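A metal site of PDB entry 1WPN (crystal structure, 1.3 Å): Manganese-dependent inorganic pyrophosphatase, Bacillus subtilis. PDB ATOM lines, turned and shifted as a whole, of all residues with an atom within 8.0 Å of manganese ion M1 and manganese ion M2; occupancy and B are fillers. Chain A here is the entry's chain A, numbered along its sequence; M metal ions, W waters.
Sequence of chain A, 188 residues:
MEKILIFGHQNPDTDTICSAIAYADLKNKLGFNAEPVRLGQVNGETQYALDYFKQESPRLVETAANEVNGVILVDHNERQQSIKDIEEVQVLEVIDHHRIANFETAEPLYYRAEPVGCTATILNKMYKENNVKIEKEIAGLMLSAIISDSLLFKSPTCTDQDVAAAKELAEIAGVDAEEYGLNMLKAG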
ATOM      1  N   GLY A   8       1.373  27.350  16.772  1.00  0.00           N
ATOM      2  CA  GLY A   8       2.402  28.332  16.514  1.00  0.00           C
ATOM      3  C   GLY A   8       1.924  29.750  16.772  1.00  0.00           C
ATOM      4  O   GLY A   8       0.987  29.985  17.578  1.00  0.00           O
ATOM      5  N   HIS A   9       2.633  30.690  16.152  1.00  0.00           N
ATOM      6  CA  HIS A   9       2.441  32.094  16.525  1.00  0.00           C
ATOM      7  C   HIS A   9       1.223  32.783  15.883  1.00  0.00           C
ATOM      8  O   HIS A   9       0.637  32.300  14.905  1.00  0.00           O
ATOM      9  CB  HIS A   9       3.706  32.936  16.228  1.00  0.00           C
ATOM     10  CG  HIS A   9       4.289  32.745  14.839  1.00  0.00           C
ATOM     11  ND1 HIS A   9       3.687  33.248  13.702  1.00  0.00           N
ATOM     12  CD2 HIS A   9       5.408  32.097  14.420  1.00  0.00           C
ATOM     13  CE1 HIS A   9       4.417  32.918  12.637  1.00  0.00           C
ATOM     14  NE2 HIS A   9       5.476  32.221  13.039  1.00  0.00           N
ATOM     15  N   GLN A  10       0.888  33.950  16.429  1.00  0.00           N
ATOM     16  CA  GLN A  10      -0.042  34.910  15.784  1.00  0.00           C
ATOM     17  C   GLN A  10       0.518  35.282  14.429  1.00  0.00           C
ATOM     18  O   GLN A  10       1.730  35.224  14.229  1.00  0.00           O
ATOM     19  CB  GLN A  10      -0.135  36.204  16.608  1.00  0.00           C
ATOM     20  CG  GLN A  10      -0.747  36.039  17.969  1.00  0.00           C
ATOM     21  CD  GLN A  10      -0.932  37.368  18.702  1.00  0.00           C
ATOM     22  OE1 GLN A  10      -1.475  38.344  18.121  1.00  0.00           O
ATOM     23  NE2 GLN A  10      -0.562  37.402  19.969  1.00  0.00           N
ATOM     24  N   ASN A  11      -0.348  35.729  13.519  1.00  0.00           N
ATOM     25  CA  ASN A  11       0.043  35.980  12.122  1.00  0.00           C
ATOM     26  C   ASN A  11       0.722  34.738  11.520  1.00  0.00           C
ATOM     27  O   ASN A  11       1.924  34.725  11.211  1.00  0.00           O
ATOM     28  CB  ASN A  11       0.916  37.239  11.986  1.00  0.00           C
ATOM     29  CG  ASN A  11       0.237  38.456  12.534  1.00  0.00           C
ATOM     30  OD1 ASN A  11      -0.959  38.711  12.261  1.00  0.00           O
ATOM     31  ND2 ASN A  11       0.991  39.243  13.300  1.00  0.00           N
ATOM     32  N   PRO A  12      -0.021  33.644  11.463  1.00  0.00           N
ATOM     33  CA  PRO A  12       0.628  32.357  11.147  1.00  0.00           C
ATOM     34  C   PRO A  12       1.323  32.312   9.805  1.00  0.00           C
ATOM     35  O   PRO A  12       0.777  32.893   8.808  1.00  0.00           O
ATOM     36  CB  PRO A  12      -0.531  31.353  11.136  1.00  0.00           C
ATOM     37  CG  PRO A  12      -1.769  32.125  11.368  1.00  0.00           C
ATOM     38  CD  PRO A  12      -1.455  33.500  11.757  1.00  0.00           C
ATOM     39  N   ASP A  13       2.479  31.636   9.776  1.00  0.00           N
ATOM     40  CA  ASP A  13       3.118  31.313   8.523  1.00  0.00           C
ATOM     41  C   ASP A  13       3.006  29.794   8.322  1.00  0.00           C
ATOM     42  O   ASP A  13       2.474  29.060   9.179  1.00  0.00           O
ATOM     43  CB  ASP A  13       4.590  31.832   8.475  1.00  0.00           C
ATOM     44  CG  ASP A  13       5.384  31.437   9.696  1.00  0.00           C
ATOM     45  OD1 ASP A  13       6.394  32.164  10.068  1.00  0.00           O
ATOM     46  OD2 ASP A  13       5.144  30.382  10.326  1.00  0.00           O
ATOM     47  N   THR A  14       3.548  29.332   7.211  1.00  0.00           N
ATOM     48  CA  THR A  14       3.422  27.947   6.840  1.00  0.00           C
ATOM     49  C   THR A  14       4.084  27.032   7.876  1.00  0.00           C
ATOM     50  O   THR A  14       3.532  25.987   8.213  1.00  0.00           O
ATOM     51  CB  THR A  14       3.999  27.748   5.450  1.00  0.00           C
ATOM     52  OG1 THR A  14       3.224  28.481   4.527  1.00  0.00           O
ATOM     53  CG2 THR A  14       3.973  26.269   4.982  1.00  0.00           C
ATOM     54  N   ASP A  15       5.253  27.411   8.425  1.00  0.00           N
ATOM     55  CA  ASP A  15       5.885  26.571   9.435  1.00  0.00           C
ATOM     56  C   ASP A  15       4.965  26.475  10.663  1.00  0.00           C
ATOM     57  O   ASP A  15       4.830  25.406  11.257  1.00  0.00           O
ATOM     58  CB  ASP A  15       7.243  27.146   9.803  1.00  0.00           C
ATOM     59  CG  ASP A  15       8.066  26.233  10.671  1.00  0.00           C
ATOM     60  OD1 ASP A  15       7.891  24.985  10.605  1.00  0.00           O
ATOM     61  OD2 ASP A  15       8.957  26.723  11.403  1.00  0.00           O
ATOM     62  N   THR A  16       4.403  27.602  11.096  1.00  0.00           N
ATOM     63  CA  THR A  16       3.578  27.585  12.288  1.00  0.00           C
ATOM     64  C   THR A  16       2.323  26.742  12.128  1.00  0.00           C
ATOM     65  O   THR A  16       1.878  26.129  13.115  1.00  0.00           O
ATOM     66  CB  THR A  16       3.263  29.057  12.680  1.00  0.00           C
ATOM     67  OG1 THR A  16       4.043  29.434  13.809  1.00  0.00           O
ATOM     68  CG2 THR A  16       1.796  29.311  13.057  1.00  0.00           C
ATOM     69  N   ILE A  17       1.755  26.695  10.920  1.00  0.00           N
ATOM     70  CA  ILE A  17       0.580  25.841  10.731  1.00  0.00           C
ATOM     71  C   ILE A  17       0.992  24.373  10.569  1.00  0.00           C
ATOM     72  O   ILE A  17       0.449  23.482  11.231  1.00  0.00           O
ATOM     73  CB  ILE A  17      -0.199  26.358   9.475  1.00  0.00           C
ATOM     74  CG1 ILE A  17      -0.756  27.785   9.711  1.00  0.00           C
ATOM     75  CG2 ILE A  17      -1.251  25.360   9.064  1.00  0.00           C
ATOM     76  CD1 ILE A  17      -1.806  27.892  10.821  1.00  0.00           C
ATOM     77  N   SER A  19       3.843  22.771  11.271  1.00  0.00           N
ATOM     78  CA  SER A  19       4.512  22.137  12.403  1.00  0.00           C
ATOM     79  C   SER A  19       3.516  21.835  13.523  1.00  0.00           C
ATOM     80  O   SER A  19       3.700  20.866  14.231  1.00  0.00           O
ATOM     81  CB  SER A  19       5.641  22.995  12.922  1.00  0.00           C
ATOM     82  OG  SER A  19       6.737  22.906  12.026  1.00  0.00           O
ATOM     83  N   VAL A  74       4.835  25.587  19.082  1.00  0.00           N
ATOM     84  CA  VAL A  74       5.786  25.308  17.997  1.00  0.00           C
ATOM     85  C   VAL A  74       6.155  26.614  17.336  1.00  0.00           C
ATOM     86  O   VAL A  74       5.303  27.533  17.229  1.00  0.00           O
ATOM     87  CB  VAL A  74       5.219  24.306  16.959  1.00  0.00           C
ATOM     88  CG1 VAL A  74       5.060  22.935  17.646  1.00  0.00           C
ATOM     89  CG2 VAL A  74       3.905  24.758  16.344  1.00  0.00           C
ATOM     90  N   ASP A  75       7.407  26.705  16.854  1.00  0.00           N
ATOM     91  CA  ASP A  75       7.841  27.803  15.995  1.00  0.00           C
ATOM     92  C   ASP A  75       7.833  29.170  16.679  1.00  0.00           C
ATOM     93  O   ASP A  75       7.971  30.197  15.989  1.00  0.00           O
ATOM     94  CB  ASP A  75       6.967  27.850  14.698  1.00  0.00           C
ATOM     95  CG  ASP A  75       7.523  28.756  13.663  1.00  0.00           C
ATOM     96  OD1 ASP A  75       6.735  29.518  13.027  1.00  0.00           O
ATOM     97  OD2 ASP A  75       8.764  28.716  13.408  1.00  0.00           O
ATOM     98  N   HIS A  76       7.711  29.208  18.000  1.00  0.00           N
ATOM     99  CA  HIS A  76       7.793  30.495  18.709  1.00  0.00           C
ATOM    100  C   HIS A  76       7.944  30.172  20.193  1.00  0.00           C
ATOM    101  O   HIS A  76       7.602  29.092  20.651  1.00  0.00           O
ATOM    102  CB  HIS A  76       6.569  31.397  18.499  1.00  0.00           C
ATOM    103  CG  HIS A  76       5.345  30.956  19.239  1.00  0.00           C
ATOM    104  ND1 HIS A  76       4.654  29.789  18.968  1.00  0.00           N
ATOM    105  CD2 HIS A  76       4.661  31.553  20.242  1.00  0.00           C
ATOM    106  CE1 HIS A  76       3.615  29.672  19.787  1.00  0.00           C
ATOM    107  NE2 HIS A  76       3.570  30.734  20.560  1.00  0.00           N
ATOM    108  N   GLN A  81       4.151  36.866  20.730  1.00  0.00           N
ATOM    109  CA  GLN A  81       3.840  36.102  19.507  1.00  0.00           C
ATOM    110  C   GLN A  81       2.835  34.985  19.793  1.00  0.00           C
ATOM    111  O   GLN A  81       2.371  34.332  18.865  1.00  0.00           O
ATOM    112  CB  GLN A  81       5.103  35.483  18.910  1.00  0.00           C
ATOM    113  CG  GLN A  81       6.123  36.537  18.476  1.00  0.00           C
ATOM    114  CD  GLN A  81       7.403  35.900  17.962  1.00  0.00           C
ATOM    115  OE1 GLN A  81       7.488  34.665  17.816  1.00  0.00           O
ATOM    116  NE2 GLN A  81       8.438  36.732  17.698  1.00  0.00           N
ATOM    117  N   ILE A  95       8.847  23.620  20.802  1.00  0.00           N
ATOM    118  CA  ILE A  95       9.772  23.152  19.752  1.00  0.00           C
ATOM    119  C   ILE A  95      10.023  24.350  18.845  1.00  0.00           C
ATOM    120  O   ILE A  95       9.050  24.840  18.279  1.00  0.00           O
ATOM    121  CB  ILE A  95       9.188  21.971  18.904  1.00  0.00           C
ATOM    122  CG1 ILE A  95       8.480  20.920  19.786  1.00  0.00           C
ATOM    123  CG2 ILE A  95      10.305  21.361  18.061  1.00  0.00           C
ATOM    124  CD1 ILE A  95       9.373  20.169  20.756  1.00  0.00           C
ATOM    125  N   ASP A  96      11.244  24.816  18.699  1.00  0.00           N
ATOM    126  CA  ASP A  96      11.448  26.129  18.023  1.00  0.00           C
ATOM    127  C   ASP A  96      12.861  26.249  17.468  1.00  0.00           C
ATOM    128  O   ASP A  96      13.739  25.436  17.735  1.00  0.00           O
ATOM    129  CB  ASP A  96      11.190  27.249  19.075  1.00  0.00           C
ATOM    130  CG  ASP A  96      11.161  28.621  18.461  1.00  0.00           C
ATOM    131  OD1 ASP A  96      11.562  29.579  19.161  1.00  0.00           O
ATOM    132  OD2 ASP A  96      10.703  28.770  17.304  1.00  0.00           O
ATOM    133  N   HIS A  97      13.059  27.298  16.668  1.00  0.00           N
ATOM    134  CA  HIS A  97      14.344  27.539  16.025  1.00  0.00           C
ATOM    135  C   HIS A  97      14.748  29.009  16.104  1.00  0.00           C
ATOM    136  O   HIS A  97      15.527  29.473  15.306  1.00  0.00           O
ATOM    137  CB  HIS A  97      14.334  27.021  14.554  1.00  0.00           C
ATOM    138  CG  HIS A  97      13.383  27.748  13.643  1.00  0.00           C
ATOM    139  ND1 HIS A  97      13.823  28.634  12.667  1.00  0.00           N
ATOM    140  CD2 HIS A  97      12.025  27.701  13.501  1.00  0.00           C
ATOM    141  CE1 HIS A  97      12.780  29.059  11.950  1.00  0.00           C
ATOM    142  NE2 HIS A  97      11.676  28.519  12.442  1.00  0.00           N
ATOM    143  N   HIS A  98      14.231  29.738  17.109  1.00  0.00           N
ATOM    144  CA  HIS A  98      14.504  31.170  17.264  1.00  0.00           C
ATOM    145  C   HIS A  98      15.250  31.476  18.532  1.00  0.00           C
ATOM    146  O   HIS A  98      15.405  30.609  19.421  1.00  0.00           O
ATOM    147  CB  HIS A  98      13.165  31.946  17.245  1.00  0.00           C
ATOM    148  CG  HIS A  98      12.387  31.784  15.979  1.00  0.00           C
ATOM    149  ND1 HIS A  98      11.390  30.859  15.840  1.00  0.00           N
ATOM    150  CD2 HIS A  98      12.524  32.389  14.768  1.00  0.00           C
ATOM    151  CE1 HIS A  98      10.890  30.921  14.595  1.00  0.00           C
ATOM    152  NE2 HIS A  98      11.580  31.848  13.930  1.00  0.00           N
ATOM    153  N   VAL A 116      18.513  25.847  13.510  1.00  0.00           N
ATOM    154  CA  VAL A 116      18.225  25.500  12.127  1.00  0.00           C
ATOM    155  C   VAL A 116      17.202  26.473  11.540  1.00  0.00           C
ATOM    156  O   VAL A 116      16.678  27.372  12.258  1.00  0.00           O
ATOM    157  CB  VAL A 116      17.715  24.050  12.004  1.00  0.00           C
ATOM    158  CG1 VAL A 116      18.800  23.079  12.448  1.00  0.00           C
ATOM    159  CG2 VAL A 116      16.433  23.814  12.831  1.00  0.00           C
ATOM    160  N   GLY A 117      16.905  26.296  10.248  1.00  0.00           N
ATOM    161  CA  GLY A 117      16.072  27.289   9.602  1.00  0.00           C
ATOM    162  C   GLY A 117      14.579  27.054   9.661  1.00  0.00           C
ATOM    163  O   GLY A 117      13.847  27.913   9.188  1.00  0.00           O
ATOM    164  N   CYS A 118      14.121  25.966  10.282  1.00  0.00           N
ATOM    165  CA  CYS A 118      12.675  25.668  10.260  1.00  0.00           C
ATOM    166  C   CYS A 118      12.328  24.701  11.362  1.00  0.00           C
ATOM    167  O   CYS A 118      13.112  23.791  11.633  1.00  0.00           O
ATOM    168  CB  CYS A 118      12.336  25.006   8.892  1.00  0.00           C
ATOM    169  SG  CYS A 118      10.591  24.662   8.673  1.00  0.00           S
ATOM    170  N   THR A 119      11.158  24.866  11.991  1.00  0.00           N
ATOM    171  CA  THR A 119      10.756  23.921  13.057  1.00  0.00           C
ATOM    172  C   THR A 119      10.590  22.515  12.524  1.00  0.00           C
ATOM    173  O   THR A 119      10.904  21.522  13.219  1.00  0.00           O
ATOM    174  CB  THR A 119       9.426  24.360  13.672  1.00  0.00           C
ATOM    175  OG1 THR A 119       9.571  25.726  14.115  1.00  0.00           O
ATOM    176  CG2 THR A 119       9.088  23.491  14.910  1.00  0.00           C
ATOM    177  N   ALA A 120      10.152  22.402  11.267  1.00  0.00           N
ATOM    178  CA  ALA A 120       9.844  21.072  10.721  1.00  0.00           C
ATOM    179  C   ALA A 120      11.126  20.198  10.586  1.00  0.00           C
ATOM    180  O   ALA A 120      11.018  18.973  10.646  1.00  0.00           O
ATOM    181  CB  ALA A 120       9.149  21.214   9.393  1.00  0.00           C
ATOM    182  N   ALA A 145       6.775  23.626   5.041  1.00  0.00           N
ATOM    183  CA  ALA A 145       7.343  24.490   6.082  1.00  0.00           C
ATOM    184  C   ALA A 145       8.817  24.849   5.811  1.00  0.00           C
ATOM    185  O   ALA A 145       9.167  26.033   5.897  1.00  0.00           O
ATOM    186  CB  ALA A 145       7.253  23.774   7.419  1.00  0.00           C
ATOM    187  N   ILE A 146       9.629  23.873   5.425  1.00  0.00           N
ATOM    188  CA  ILE A 146      11.029  24.145   5.162  1.00  0.00           C
ATOM    189  C   ILE A 146      11.192  25.029   3.948  1.00  0.00           C
ATOM    190  O   ILE A 146      11.989  25.956   3.984  1.00  0.00           O
ATOM    191  CB  ILE A 146      11.772  22.829   4.959  1.00  0.00           C
ATOM    192  CG1 ILE A 146      11.775  21.997   6.257  1.00  0.00           C
ATOM    193  CG2 ILE A 146      13.266  23.077   4.524  1.00  0.00           C
ATOM    194  CD1 ILE A 146      12.186  20.549   6.117  1.00  0.00           C
ATOM    195  N   SER A 148       9.060  27.224   2.821  1.00  0.00           N
ATOM    196  CA  SER A 148       8.592  28.516   3.218  1.00  0.00           C
ATOM    197  C   SER A 148       9.610  29.302   4.057  1.00  0.00           C
ATOM    198  O   SER A 148       9.967  30.433   3.710  1.00  0.00           O
ATOM    199  CB  SER A 148       7.307  28.360   4.024  1.00  0.00           C
ATOM    200  OG  SER A 148       6.888  29.626   4.497  1.00  0.00           O
ATOM    201  N   ASP A 149      10.110  28.664   5.121  1.00  0.00           N
ATOM    202  CA  ASP A 149      11.058  29.371   5.980  1.00  0.00           C
ATOM    203  C   ASP A 149      12.388  29.623   5.316  1.00  0.00           C
ATOM    204  O   ASP A 149      13.031  30.651   5.583  1.00  0.00           O
ATOM    205  CB  ASP A 149      11.275  28.616   7.270  1.00  0.00           C
ATOM    206  CG  ASP A 149      10.307  28.958   8.350  1.00  0.00           C
ATOM    207  OD1 ASP A 149       9.442  29.840   8.226  1.00  0.00           O
ATOM    208  OD2 ASP A 149      10.390  28.340   9.441  1.00  0.00           O
ATOM    209  N   SER A 150      12.802  28.709   4.456  1.00  0.00           N
ATOM    210  CA  SER A 150      14.108  28.856   3.785  1.00  0.00           C
ATOM    211  C   SER A 150      14.018  29.670   2.502  1.00  0.00           C
ATOM    212  O   SER A 150      15.068  29.895   1.882  1.00  0.00           O
ATOM    213  CB  SER A 150      14.706  27.499   3.493  1.00  0.00           C
ATOM    214  OG  SER A 150      14.007  26.912   2.392  1.00  0.00           O
HETATM  215 MN    MN M   1       9.727  28.711  11.470  1.00  0.00          MN
HETATM  216 MN    MN M   2       7.134  31.281  11.855  1.00  0.00          MN
HETATM  217  O   HOH W   1       8.804  30.418  10.886  1.00  0.00           O
HETATM  218  O   HOH W   2       8.425  32.496  13.075  1.00  0.00           O
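The backbone NH (N) of Thr 16 lies close to the side-chain carboxylate (OD2) of Asp 13 (3.0 Å).
The side-chain carboxylate (OD1) of Asp 15 lies within hydrogen-bond range of the backbone NH (N) of Ala 120 (3.5 Å).
OD2 of Asp 75 lies close to OG1 of Thr 119.
O of Asp 75 lies close to ND1 of His 98 (3.5 Å).
The side-chain carboxylate of Asp 75 sits close to the side-chain hydroxyl of Thr 16 (2.8 Å).
The backbone NH of Asp 75 sits at hydrogen-bond distance from the backbone carbonyl oxygen of Ile 95, 2.9 Å away.
The side-chain sulfur (SG) of Cys 118 sits close to the side-chain carboxylate (OD2) of Asp 149.
A ring nitrogen (ND1) of His 9 sits at hydrogen-bond distance from the backbone carbonyl oxygen (O) of Asn 11, 3.4 Å away.
Merely in contact with manganese ion M1: Thr 119.
Within 4 Å of manganese ion M1: Asp 15, Asp 75, His 97, Thr 119 and Asp 149.
The nearest printed residue that does not touch manganese ion M1 is His 98 (4.0003 Å).
Within 4 Å of manganese ion M2: His 9, Asp 13 and Asp 75.
Water W1 is bound to manganese ion M1.
The side-chain carboxylate (OD2) of Asp 15 binds manganese ion M1.
OD2 of Asp 75 binds manganese ion M1, at 2.2 Å.
The side-chain carboxylate (OD2) of Asp 149 binds manganese ion M1 (2.2 Å).
NE2 of His 97 binds manganese ion M1.
Manganese ion M1 has five donor atoms within binding distance.
Manganese ion M2 is bound by water W1 (2.1 Å), OD1 of Asp 13 (2.1 Å), water W2 (2.2 Å), OD1 of Asp 75 (2.2 Å), NE2 of His 9 (2.2 Å) and OD2 of Asp 13 (2.7 Å).
Manganese ion M2 has six donor atoms within binding distance.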
